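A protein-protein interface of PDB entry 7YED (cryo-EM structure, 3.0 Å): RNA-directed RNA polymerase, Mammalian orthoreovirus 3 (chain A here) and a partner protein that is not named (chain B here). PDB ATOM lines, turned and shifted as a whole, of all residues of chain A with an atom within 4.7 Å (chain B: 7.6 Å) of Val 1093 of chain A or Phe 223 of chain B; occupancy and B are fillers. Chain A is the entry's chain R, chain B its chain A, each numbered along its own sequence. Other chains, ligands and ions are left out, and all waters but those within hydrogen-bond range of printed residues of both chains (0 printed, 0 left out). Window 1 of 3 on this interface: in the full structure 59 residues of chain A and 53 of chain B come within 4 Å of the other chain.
The indole nitrogen (NE1) of Trp 227 of chain B lies within hydrogen-bond range of the side-chain carboxylate (OD1) of Asp 1072 of chain A (3.3 Å).
The backbone carbonyl oxygen (O) of Pro 1069 of chain A sits at hydrogen-bond distance from the backbone NH (N) of Asn 585 of chain B, 3.1 Å away.
The guanidinium group (NH2) of Arg 218 of chain B sits at hydrogen-bond distance from a ring nitrogen (NE2) of His 219 of chain B, 3.1 Å away.
The guanidinium group (NH1) of Arg 218 of chain B is in salt-bridge range of the side-chain carboxylate (OE2) of Glu 222 of chain B, at 3.1 Å.
O of Ser 1094 of chain A is in hydrogen-bond range of NE of Arg 1067 of chain A (3.3 Å).
N of Ser 1070 of chain A is in hydrogen-bond range of O of Val 1093 of chain A (3.2 Å).
O of Leu 1090 of chain A is in hydrogen-bond range of OG of Ser 1094 of chain A (2.7 Å).
His 219 of chain B touches Ala 1066 of chain A (O to CB, 3.5 Å).
OE1 of Glu 222 of chain B touches N of Ala 1066 of chain A (3.5 Å).
Glu 1068 of chain A touches Phe 223 of chain B.
Pro 1069 of chain A touches Phe 223 of chain B (CG to CZ, 3.5 Å).
Pro 1069 of chain A touches Trp 227 of chain B (CG to CB, 3.97 Å).
CG of Trp 227 of chain B touches CD1 of Leu 1073 of chain A (3.7 Å).
O of Val 1093 of chain A touches CZ of Phe 223 of chain B, 3.95 Å away.
Phe 223 of chain B touches Ser 1094 of chain A.
Val 1236 of chain A touches His 219 of chain B (CG2 to O, 3.8 Å).
Phe 223 of chain B touches Val 1236 of chain A.
Of chain B, only Phe 223 comes within 4 Å of Val 1093 of chain A.
Of chain A, only Ala 1066 (3.9 Å), Arg 1067 (3.0 Å), Glu 1068 (3.9 Å), Pro 1069 (3.5 Å), Val 1093 (3.95 Å), Ser 1094 (3.6 Å) and Val 1236 (3.9 Å) come within 4 Å of Phe 223 of chain B.
Printed residues of chain B within 4 Å of Ala 1066 of chain A: His 219, Glu 222 and Phe 223.
Of the printed residues of chain B, Val 1236 of chain A touches His 219 (3.8 Å) and Phe 223 (3.9 Å).
Printed residues of chain B within 4 Å of Ser 1094 of chain A: Phe 223 (3.6 Å).
Of the 15 printed residues of chain B, 5 touch a printed residue of chain A.
Hydrophobic or aromatic side chains of chain B within 4 Å of the printed part of chain A: His 219, Phe 223 and Trp 227.
Of the 17 printed residues of chain A, 9 touch a printed residue of chain B.
Among the printed residues, no Asp or Glu carboxylate lies within 4 Å of a Lys or Arg side-chain nitrogen of the other chain.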
ATOM      1  N   ALA A1066      -9.970  20.757   9.129  1.00  0.00           N
ATOM      2  CA  ALA A1066      -9.484  19.617   8.366  1.00  0.00           C
ATOM      3  C   ALA A1066      -9.094  20.082   6.971  1.00  0.00           C
ATOM      4  O   ALA A1066      -9.927  20.620   6.235  1.00  0.00           O
ATOM      5  CB  ALA A1066     -10.550  18.528   8.294  1.00  0.00           C
ATOM      6  N   ARG A1067      -7.830  19.888   6.611  1.00  0.00           N
ATOM      7  CA  ARG A1067      -7.364  20.275   5.292  1.00  0.00           C
ATOM      8  C   ARG A1067      -8.061  19.449   4.215  1.00  0.00           C
ATOM      9  O   ARG A1067      -8.552  18.345   4.462  1.00  0.00           O
ATOM     10  CB  ARG A1067      -5.849  20.109   5.194  1.00  0.00           C
ATOM     11  CG  ARG A1067      -5.378  18.692   5.422  1.00  0.00           C
ATOM     12  CD  ARG A1067      -3.870  18.590   5.330  1.00  0.00           C
ATOM     13  NE  ARG A1067      -3.391  18.788   3.969  1.00  0.00           N
ATOM     14  CZ  ARG A1067      -2.120  18.994   3.650  1.00  0.00           C
ATOM     15  NH1 ARG A1067      -1.200  19.029   4.601  1.00  0.00           N
ATOM     16  NH2 ARG A1067      -1.767  19.161   2.384  1.00  0.00           N
ATOM     17  N   GLU A1068      -8.110  20.003   3.008  1.00  0.00           N
ATOM     18  CA  GLU A1068      -8.779  19.334   1.910  1.00  0.00           C
ATOM     19  C   GLU A1068      -8.031  18.060   1.532  1.00  0.00           C
ATOM     20  O   GLU A1068      -6.835  17.928   1.795  1.00  0.00           O
ATOM     21  CB  GLU A1068      -8.879  20.262   0.707  1.00  0.00           C
ATOM     22  CG  GLU A1068      -9.796  21.448   0.924  1.00  0.00           C
ATOM     23  CD  GLU A1068      -9.853  22.368  -0.276  1.00  0.00           C
ATOM     24  OE1 GLU A1068      -9.070  22.157  -1.226  1.00  0.00           O
ATOM     25  OE2 GLU A1068     -10.682  23.301  -0.271  1.00  0.00           O
ATOM     26  N   PRO A1069      -8.721  17.102   0.916  1.00  0.00           N
ATOM     27  CA  PRO A1069      -8.068  15.839   0.561  1.00  0.00           C
ATOM     28  C   PRO A1069      -6.974  16.058  -0.470  1.00  0.00           C
ATOM     29  O   PRO A1069      -7.056  16.952  -1.311  1.00  0.00           O
ATOM     30  CB  PRO A1069      -9.210  14.997  -0.014  1.00  0.00           C
ATOM     31  CG  PRO A1069     -10.442  15.599   0.550  1.00  0.00           C
ATOM     32  CD  PRO A1069     -10.162  17.066   0.634  1.00  0.00           C
ATOM     33  N   SER A1070      -5.938  15.228  -0.391  1.00  0.00           N
ATOM     34  CA  SER A1070      -4.830  15.285  -1.335  1.00  0.00           C
ATOM     35  C   SER A1070      -4.759  14.049  -2.217  1.00  0.00           C
ATOM     36  O   SER A1070      -3.763  13.853  -2.918  1.00  0.00           O
ATOM     37  CB  SER A1070      -3.510  15.479  -0.592  1.00  0.00           C
ATOM     38  OG  SER A1070      -3.487  16.731   0.063  1.00  0.00           O
ATOM     39  N   VAL A1071      -5.786  13.206  -2.190  1.00  0.00           N
ATOM     40  CA  VAL A1071      -5.868  12.053  -3.074  1.00  0.00           C
ATOM     41  C   VAL A1071      -7.295  11.533  -3.018  1.00  0.00           C
ATOM     42  O   VAL A1071      -7.999  11.739  -2.025  1.00  0.00           O
ATOM     43  CB  VAL A1071      -4.854  10.966  -2.681  1.00  0.00           C
ATOM     44  CG1 VAL A1071      -5.216  10.368  -1.341  1.00  0.00           C
ATOM     45  CG2 VAL A1071      -4.790   9.892  -3.744  1.00  0.00           C
ATOM     46  N   ASP A1072      -7.741  10.874  -4.081  1.00  0.00           N
ATOM     47  CA  ASP A1072      -9.109  10.377  -4.122  1.00  0.00           C
ATOM     48  C   ASP A1072      -9.307   9.282  -3.082  1.00  0.00           C
ATOM     49  O   ASP A1072      -8.414   8.469  -2.834  1.00  0.00           O
ATOM     50  CB  ASP A1072      -9.436   9.850  -5.514  1.00  0.00           C
ATOM     51  CG  ASP A1072     -10.894   9.483  -5.667  1.00  0.00           C
ATOM     52  OD1 ASP A1072     -11.727  10.405  -5.773  1.00  0.00           O
ATOM     53  OD2 ASP A1072     -11.210   8.276  -5.684  1.00  0.00           O
ATOM     54  N   LEU A1073     -10.486   9.266  -2.469  1.00  0.00           N
ATOM     55  CA  LEU A1073     -10.808   8.283  -1.444  1.00  0.00           C
ATOM     56  C   LEU A1073     -11.279   6.956  -2.021  1.00  0.00           C
ATOM     57  O   LEU A1073     -11.765   6.109  -1.268  1.00  0.00           O
ATOM     58  CB  LEU A1073     -11.872   8.836  -0.499  1.00  0.00           C
ATOM     59  CG  LEU A1073     -11.398   9.812   0.574  1.00  0.00           C
ATOM     60  CD1 LEU A1073     -11.023  11.143  -0.036  1.00  0.00           C
ATOM     61  CD2 LEU A1073     -12.476   9.994   1.621  1.00  0.00           C
ATOM     62  N   PHE A1089      -5.326   4.977   6.566  1.00  0.00           N
ATOM     63  CA  PHE A1089      -6.084   5.429   5.408  1.00  0.00           C
ATOM     64  C   PHE A1089      -6.340   6.926   5.471  1.00  0.00           C
ATOM     65  O   PHE A1089      -6.133   7.645   4.488  1.00  0.00           O
ATOM     66  CB  PHE A1089      -7.398   4.665   5.321  1.00  0.00           C
ATOM     67  CG  PHE A1089      -8.235   5.047   4.145  1.00  0.00           C
ATOM     68  CD1 PHE A1089      -7.900   4.621   2.879  1.00  0.00           C
ATOM     69  CD2 PHE A1089      -9.360   5.827   4.306  1.00  0.00           C
ATOM     70  CE1 PHE A1089      -8.668   4.968   1.798  1.00  0.00           C
ATOM     71  CE2 PHE A1089     -10.130   6.174   3.225  1.00  0.00           C
ATOM     72  CZ  PHE A1089      -9.784   5.744   1.971  1.00  0.00           C
ATOM     73  N   LEU A1090      -6.790   7.416   6.625  1.00  0.00           N
ATOM     74  CA  LEU A1090      -7.077   8.839   6.751  1.00  0.00           C
ATOM     75  C   LEU A1090      -5.809   9.671   6.610  1.00  0.00           C
ATOM     76  O   LEU A1090      -5.819  10.710   5.940  1.00  0.00           O
ATOM     77  CB  LEU A1090      -7.766   9.119   8.082  1.00  0.00           C
ATOM     78  CG  LEU A1090      -9.158   8.505   8.217  1.00  0.00           C
ATOM     79  CD1 LEU A1090      -9.708   8.728   9.609  1.00  0.00           C
ATOM     80  CD2 LEU A1090     -10.098   9.075   7.174  1.00  0.00           C
ATOM     81  N   LYS A1091      -4.706   9.224   7.212  1.00  0.00           N
ATOM     82  CA  LYS A1091      -3.455   9.962   7.081  1.00  0.00           C
ATOM     83  C   LYS A1091      -2.994  10.008   5.629  1.00  0.00           C
ATOM     84  O   LYS A1091      -2.616  11.069   5.120  1.00  0.00           O
ATOM     85  CB  LYS A1091      -2.377   9.337   7.965  1.00  0.00           C
ATOM     86  CG  LYS A1091      -2.692   9.384   9.441  1.00  0.00           C
ATOM     87  CD  LYS A1091      -2.683  10.806   9.958  1.00  0.00           C
ATOM     88  CE  LYS A1091      -2.934  10.842  11.450  1.00  0.00           C
ATOM     89  NZ  LYS A1091      -2.992  12.232  11.950  1.00  0.00           N
ATOM     90  N   MET A1092      -3.026   8.864   4.944  1.00  0.00           N
ATOM     91  CA  MET A1092      -2.585   8.814   3.554  1.00  0.00           C
ATOM     92  C   MET A1092      -3.456   9.684   2.664  1.00  0.00           C
ATOM     93  O   MET A1092      -2.949  10.401   1.797  1.00  0.00           O
ATOM     94  CB  MET A1092      -2.596   7.370   3.055  1.00  0.00           C
ATOM     95  CG  MET A1092      -2.072   7.190   1.642  1.00  0.00           C
ATOM     96  SD  MET A1092      -0.325   7.597   1.489  1.00  0.00           S
ATOM     97  CE  MET A1092       0.423   6.202   2.327  1.00  0.00           C
ATOM     98  N   VAL A1093      -4.774   9.641   2.866  1.00  0.00           N
ATOM     99  CA  VAL A1093      -5.673  10.354   1.971  1.00  0.00           C
ATOM    100  C   VAL A1093      -5.743  11.842   2.278  1.00  0.00           C
ATOM    101  O   VAL A1093      -6.089  12.629   1.390  1.00  0.00           O
ATOM    102  CB  VAL A1093      -7.075   9.735   2.024  1.00  0.00           C
ATOM    103  CG1 VAL A1093      -7.695   9.961   3.382  1.00  0.00           C
ATOM    104  CG2 VAL A1093      -7.946  10.319   0.943  1.00  0.00           C
ATOM    105  N   SER A1094      -5.422  12.263   3.501  1.00  0.00           N
ATOM    106  CA  SER A1094      -5.467  13.676   3.838  1.00  0.00           C
ATOM    107  C   SER A1094      -4.109  14.355   3.771  1.00  0.00           C
ATOM    108  O   SER A1094      -4.056  15.587   3.775  1.00  0.00           O
ATOM    109  CB  SER A1094      -6.053  13.870   5.237  1.00  0.00           C
ATOM    110  OG  SER A1094      -5.184  13.341   6.218  1.00  0.00           O
ATOM    111  N   VAL A1095      -3.017  13.598   3.722  1.00  0.00           N
ATOM    112  CA  VAL A1095      -1.688  14.159   3.546  1.00  0.00           C
ATOM    113  C   VAL A1095      -1.146  13.889   2.148  1.00  0.00           C
ATOM    114  O   VAL A1095      -0.476  14.742   1.567  1.00  0.00           O
ATOM    115  CB  VAL A1095      -0.717  13.628   4.621  1.00  0.00           C
ATOM    116  CG1 VAL A1095       0.676  14.158   4.369  1.00  0.00           C
ATOM    117  CG2 VAL A1095      -1.189  14.024   6.000  1.00  0.00           C
ATOM    118  N   GLY A1096      -1.428  12.714   1.595  1.00  0.00           N
ATOM    119  CA  GLY A1096      -0.998  12.384   0.260  1.00  0.00           C
ATOM    120  C   GLY A1096       0.360  11.720   0.246  1.00  0.00           C
ATOM    121  O   GLY A1096       1.193  11.941   1.129  1.00  0.00           O
ATOM    122  N   VAL A1236      -7.853  12.586  10.620  1.00  0.00           N
ATOM    123  CA  VAL A1236      -7.286  13.273   9.468  1.00  0.00           C
ATOM    124  C   VAL A1236      -6.331  14.355   9.944  1.00  0.00           C
ATOM    125  O   VAL A1236      -6.493  14.924  11.027  1.00  0.00           O
ATOM    126  CB  VAL A1236      -8.401  13.863   8.585  1.00  0.00           C
ATOM    127  CG1 VAL A1236      -9.294  12.762   8.064  1.00  0.00           C
ATOM    128  CG2 VAL A1236      -9.207  14.867   9.371  1.00  0.00           C
ATOM    129  N   ILE B 161     -17.557   5.358   6.923  1.00  0.00           N
ATOM    130  CA  ILE B 161     -16.743   6.567   6.837  1.00  0.00           C
ATOM    131  C   ILE B 161     -17.446   7.641   6.012  1.00  0.00           C
ATOM    132  O   ILE B 161     -17.538   8.800   6.429  1.00  0.00           O
ATOM    133  CB  ILE B 161     -15.349   6.244   6.269  1.00  0.00           C
ATOM    134  CG1 ILE B 161     -14.579   5.347   7.235  1.00  0.00           C
ATOM    135  CG2 ILE B 161     -14.577   7.519   6.024  1.00  0.00           C
ATOM    136  CD1 ILE B 161     -13.296   4.804   6.663  1.00  0.00           C
ATOM    137  N   GLN B 217     -14.446  12.812  15.258  1.00  0.00           N
ATOM    138  CA  GLN B 217     -15.617  12.784  14.387  1.00  0.00           C
ATOM    139  C   GLN B 217     -15.851  14.139  13.726  1.00  0.00           C
ATOM    140  O   GLN B 217     -16.239  14.203  12.552  1.00  0.00           O
ATOM    141  CB  GLN B 217     -16.843  12.359  15.184  1.00  0.00           C
ATOM    142  CG  GLN B 217     -16.755  10.959  15.754  1.00  0.00           C
ATOM    143  CD  GLN B 217     -16.728   9.903  14.679  1.00  0.00           C
ATOM    144  OE1 GLN B 217     -17.410  10.019  13.663  1.00  0.00           O
ATOM    145  NE2 GLN B 217     -15.939   8.862  14.895  1.00  0.00           N
ATOM    146  N   ARG B 218     -15.631  15.229  14.468  1.00  0.00           N
ATOM    147  CA  ARG B 218     -15.757  16.565  13.893  1.00  0.00           C
ATOM    148  C   ARG B 218     -14.835  16.735  12.696  1.00  0.00           C
ATOM    149  O   ARG B 218     -15.268  17.149  11.610  1.00  0.00           O
ATOM    150  CB  ARG B 218     -15.444  17.626  14.950  1.00  0.00           C
ATOM    151  CG  ARG B 218     -15.616  19.054  14.451  1.00  0.00           C
ATOM    152  CD  ARG B 218     -15.426  20.103  15.546  1.00  0.00           C
ATOM    153  NE  ARG B 218     -14.072  20.147  16.089  1.00  0.00           N
ATOM    154  CZ  ARG B 218     -13.046  20.770  15.510  1.00  0.00           C
ATOM    155  NH1 ARG B 218     -13.208  21.396  14.353  1.00  0.00           N
ATOM    156  NH2 ARG B 218     -11.852  20.763  16.087  1.00  0.00           N
ATOM    157  N   HIS B 219     -13.550  16.431  12.885  1.00  0.00           N
ATOM    158  CA  HIS B 219     -12.606  16.594  11.790  1.00  0.00           C
ATOM    159  C   HIS B 219     -12.930  15.671  10.629  1.00  0.00           C
ATOM    160  O   HIS B 219     -12.767  16.064   9.471  1.00  0.00           O
ATOM    161  CB  HIS B 219     -11.181  16.355  12.273  1.00  0.00           C
ATOM    162  CG  HIS B 219     -10.691  17.388  13.235  1.00  0.00           C
ATOM    163  ND1 HIS B 219     -10.392  18.676  12.851  1.00  0.00           N
ATOM    164  CD2 HIS B 219     -10.421  17.317  14.558  1.00  0.00           C
ATOM    165  CE1 HIS B 219      -9.971  19.358  13.901  1.00  0.00           C
ATOM    166  NE2 HIS B 219      -9.985  18.558  14.950  1.00  0.00           N
ATOM    167  N   ILE B 220     -13.415  14.460  10.906  1.00  0.00           N
ATOM    168  CA  ILE B 220     -13.718  13.543   9.814  1.00  0.00           C
ATOM    169  C   ILE B 220     -14.893  14.054   8.988  1.00  0.00           C
ATOM    170  O   ILE B 220     -14.878  13.972   7.754  1.00  0.00           O
ATOM    171  CB  ILE B 220     -13.975  12.129  10.354  1.00  0.00           C
ATOM    172  CG1 ILE B 220     -12.704  11.580  10.998  1.00  0.00           C
ATOM    173  CG2 ILE B 220     -14.436  11.219   9.237  1.00  0.00           C
ATOM    174  CD1 ILE B 220     -12.922  10.319  11.776  1.00  0.00           C
ATOM    175  N   THR B 221     -15.924  14.589   9.643  1.00  0.00           N
ATOM    176  CA  THR B 221     -17.052  15.124   8.884  1.00  0.00           C
ATOM    177  C   THR B 221     -16.641  16.348   8.074  1.00  0.00           C
ATOM    178  O   THR B 221     -17.021  16.480   6.901  1.00  0.00           O
ATOM    179  CB  THR B 221     -18.209  15.475   9.815  1.00  0.00           C
ATOM    180  OG1 THR B 221     -17.788  16.484  10.738  1.00  0.00           O
ATOM    181  CG2 THR B 221     -18.665  14.247  10.578  1.00  0.00           C
ATOM    182  N   GLU B 222     -15.871  17.255   8.686  1.00  0.00           N
ATOM    183  CA  GLU B 222     -15.375  18.414   7.949  1.00  0.00           C
ATOM    184  C   GLU B 222     -14.558  17.986   6.739  1.00  0.00           C
ATOM    185  O   GLU B 222     -14.642  18.603   5.672  1.00  0.00           O
ATOM    186  CB  GLU B 222     -14.530  19.303   8.859  1.00  0.00           C
ATOM    187  CG  GLU B 222     -15.290  19.993   9.972  1.00  0.00           C
ATOM    188  CD  GLU B 222     -14.387  20.855  10.831  1.00  0.00           C
ATOM    189  OE1 GLU B 222     -13.156  20.810  10.627  1.00  0.00           O
ATOM    190  OE2 GLU B 222     -14.901  21.579  11.707  1.00  0.00           O
ATOM    191  N   PHE B 223     -13.765  16.925   6.887  1.00  0.00           N
ATOM    192  CA  PHE B 223     -12.925  16.457   5.794  1.00  0.00           C
ATOM    193  C   PHE B 223     -13.755  15.851   4.674  1.00  0.00           C
ATOM    194  O   PHE B 223     -13.505  16.117   3.495  1.00  0.00           O
ATOM    195  CB  PHE B 223     -11.920  15.438   6.323  1.00  0.00           C
ATOM    196  CG  PHE B 223     -10.993  14.898   5.282  1.00  0.00           C
ATOM    197  CD1 PHE B 223      -9.932  15.653   4.826  1.00  0.00           C
ATOM    198  CD2 PHE B 223     -11.170  13.627   4.771  1.00  0.00           C
ATOM    199  CE1 PHE B 223      -9.073  15.155   3.877  1.00  0.00           C
ATOM    200  CE2 PHE B 223     -10.314  13.125   3.820  1.00  0.00           C
ATOM    201  CZ  PHE B 223      -9.265  13.891   3.372  1.00  0.00           C
ATOM    202  N   ILE B 224     -14.748  15.034   5.021  1.00  0.00           N
ATOM    203  CA  ILE B 224     -15.502  14.333   3.989  1.00  0.00           C
ATOM    204  C   ILE B 224     -16.504  15.238   3.283  1.00  0.00           C
ATOM    205  O   ILE B 224     -16.889  14.943   2.144  1.00  0.00           O
ATOM    206  CB  ILE B 224     -16.182  13.099   4.597  1.00  0.00           C
ATOM    207  CG1 ILE B 224     -15.115  12.121   5.070  1.00  0.00           C
ATOM    208  CG2 ILE B 224     -17.080  12.420   3.591  1.00  0.00           C
ATOM    209  CD1 ILE B 224     -15.647  11.002   5.895  1.00  0.00           C
ATOM    210  N   SER B 225     -16.918  16.345   3.902  1.00  0.00           N
ATOM    211  CA  SER B 225     -17.789  17.277   3.189  1.00  0.00           C
ATOM    212  C   SER B 225     -17.114  17.829   1.937  1.00  0.00           C
ATOM    213  O   SER B 225     -17.752  17.966   0.888  1.00  0.00           O
ATOM    214  CB  SER B 225     -18.217  18.414   4.111  1.00  0.00           C
ATOM    215  OG  SER B 225     -19.033  17.932   5.160  1.00  0.00           O
ATOM    216  N   SER B 226     -15.818  18.132   2.022  1.00  0.00           N
ATOM    217  CA  SER B 226     -15.104  18.679   0.872  1.00  0.00           C
ATOM    218  C   SER B 226     -15.022  17.663  -0.261  1.00  0.00           C
ATOM    219  O   SER B 226     -15.257  17.996  -1.432  1.00  0.00           O
ATOM    220  CB  SER B 226     -13.708  19.123   1.294  1.00  0.00           C
ATOM    221  OG  SER B 226     -13.781  20.158   2.255  1.00  0.00           O
ATOM    222  N   TRP B 227     -14.666  16.421   0.065  1.00  0.00           N
ATOM    223  CA  TRP B 227     -14.593  15.396  -0.965  1.00  0.00           C
ATOM    224  C   TRP B 227     -15.958  15.121  -1.568  1.00  0.00           C
ATOM    225  O   TRP B 227     -16.057  14.811  -2.759  1.00  0.00           O
ATOM    226  CB  TRP B 227     -13.999  14.113  -0.395  1.00  0.00           C
ATOM    227  CG  TRP B 227     -13.867  13.040  -1.415  1.00  0.00           C
ATOM    228  CD1 TRP B 227     -13.052  13.042  -2.502  1.00  0.00           C
ATOM    229  CD2 TRP B 227     -14.586  11.805  -1.455  1.00  0.00           C
ATOM    230  NE1 TRP B 227     -13.210  11.881  -3.216  1.00  0.00           N
ATOM    231  CE2 TRP B 227     -14.149  11.105  -2.592  1.00  0.00           C
ATOM    232  CE3 TRP B 227     -15.553  11.222  -0.637  1.00  0.00           C
ATOM    233  CZ2 TRP B 227     -14.647   9.855  -2.931  1.00  0.00           C
ATOM    234  CZ3 TRP B 227     -16.045   9.983  -0.976  1.00  0.00           C
ATOM    235  CH2 TRP B 227     -15.592   9.311  -2.112  1.00  0.00           C
ATOM    236  N   GLN B 228     -17.022  15.231  -0.772  1.00  0.00           N
ATOM    237  CA  GLN B 228     -18.359  15.060  -1.325  1.00  0.00           C
ATOM    238  C   GLN B 228     -18.734  16.208  -2.249  1.00  0.00           C
ATOM    239  O   GLN B 228     -19.427  15.997  -3.249  1.00  0.00           O
ATOM    240  CB  GLN B 228     -19.385  14.941  -0.201  1.00  0.00           C
ATOM    241  CG  GLN B 228     -19.228  13.706   0.654  1.00  0.00           C
ATOM    242  CD  GLN B 228     -19.450  12.432  -0.125  1.00  0.00           C
ATOM    243  OE1 GLN B 228     -18.514  11.686  -0.395  1.00  0.00           O
ATOM    244  NE2 GLN B 228     -20.699  12.174  -0.490  1.00  0.00           N
ATOM    245  N   ASN B 229     -18.293  17.424  -1.935  1.00  0.00           N
ATOM    246  CA  ASN B 229     -18.692  18.590  -2.707  1.00  0.00           C
ATOM    247  C   ASN B 229     -17.788  18.874  -3.898  1.00  0.00           C
ATOM    248  O   ASN B 229     -18.098  19.779  -4.678  1.00  0.00           O
ATOM    249  CB  ASN B 229     -18.740  19.824  -1.806  1.00  0.00           C
ATOM    250  CG  ASN B 229     -19.878  19.767  -0.815  1.00  0.00           C
ATOM    251  OD1 ASN B 229     -20.980  19.331  -1.144  1.00  0.00           O
ATOM    252  ND2 ASN B 229     -19.619  20.208   0.409  1.00  0.00           N
ATOM    253  N   ASN B 585      -8.016  17.764  -4.105  1.00  0.00           N
ATOM    254  CA  ASN B 585      -8.035  16.369  -4.539  1.00  0.00           C
ATOM    255  C   ASN B 585      -7.034  16.292  -5.632  1.00  0.00           C
ATOM    256  O   ASN B 585      -7.197  15.515  -6.552  1.00  0.00           O
ATOM    257  CB  ASN B 585      -9.396  15.905  -5.026  1.00  0.00           C
ATOM    258  CG  ASN B 585     -10.469  16.031  -3.974  1.00  0.00           C
ATOM    259  OD1 ASN B 585     -10.268  16.645  -2.930  1.00  0.00           O
ATOM    260  ND2 ASN B 585     -11.626  15.455  -4.248  1.00  0.00           N
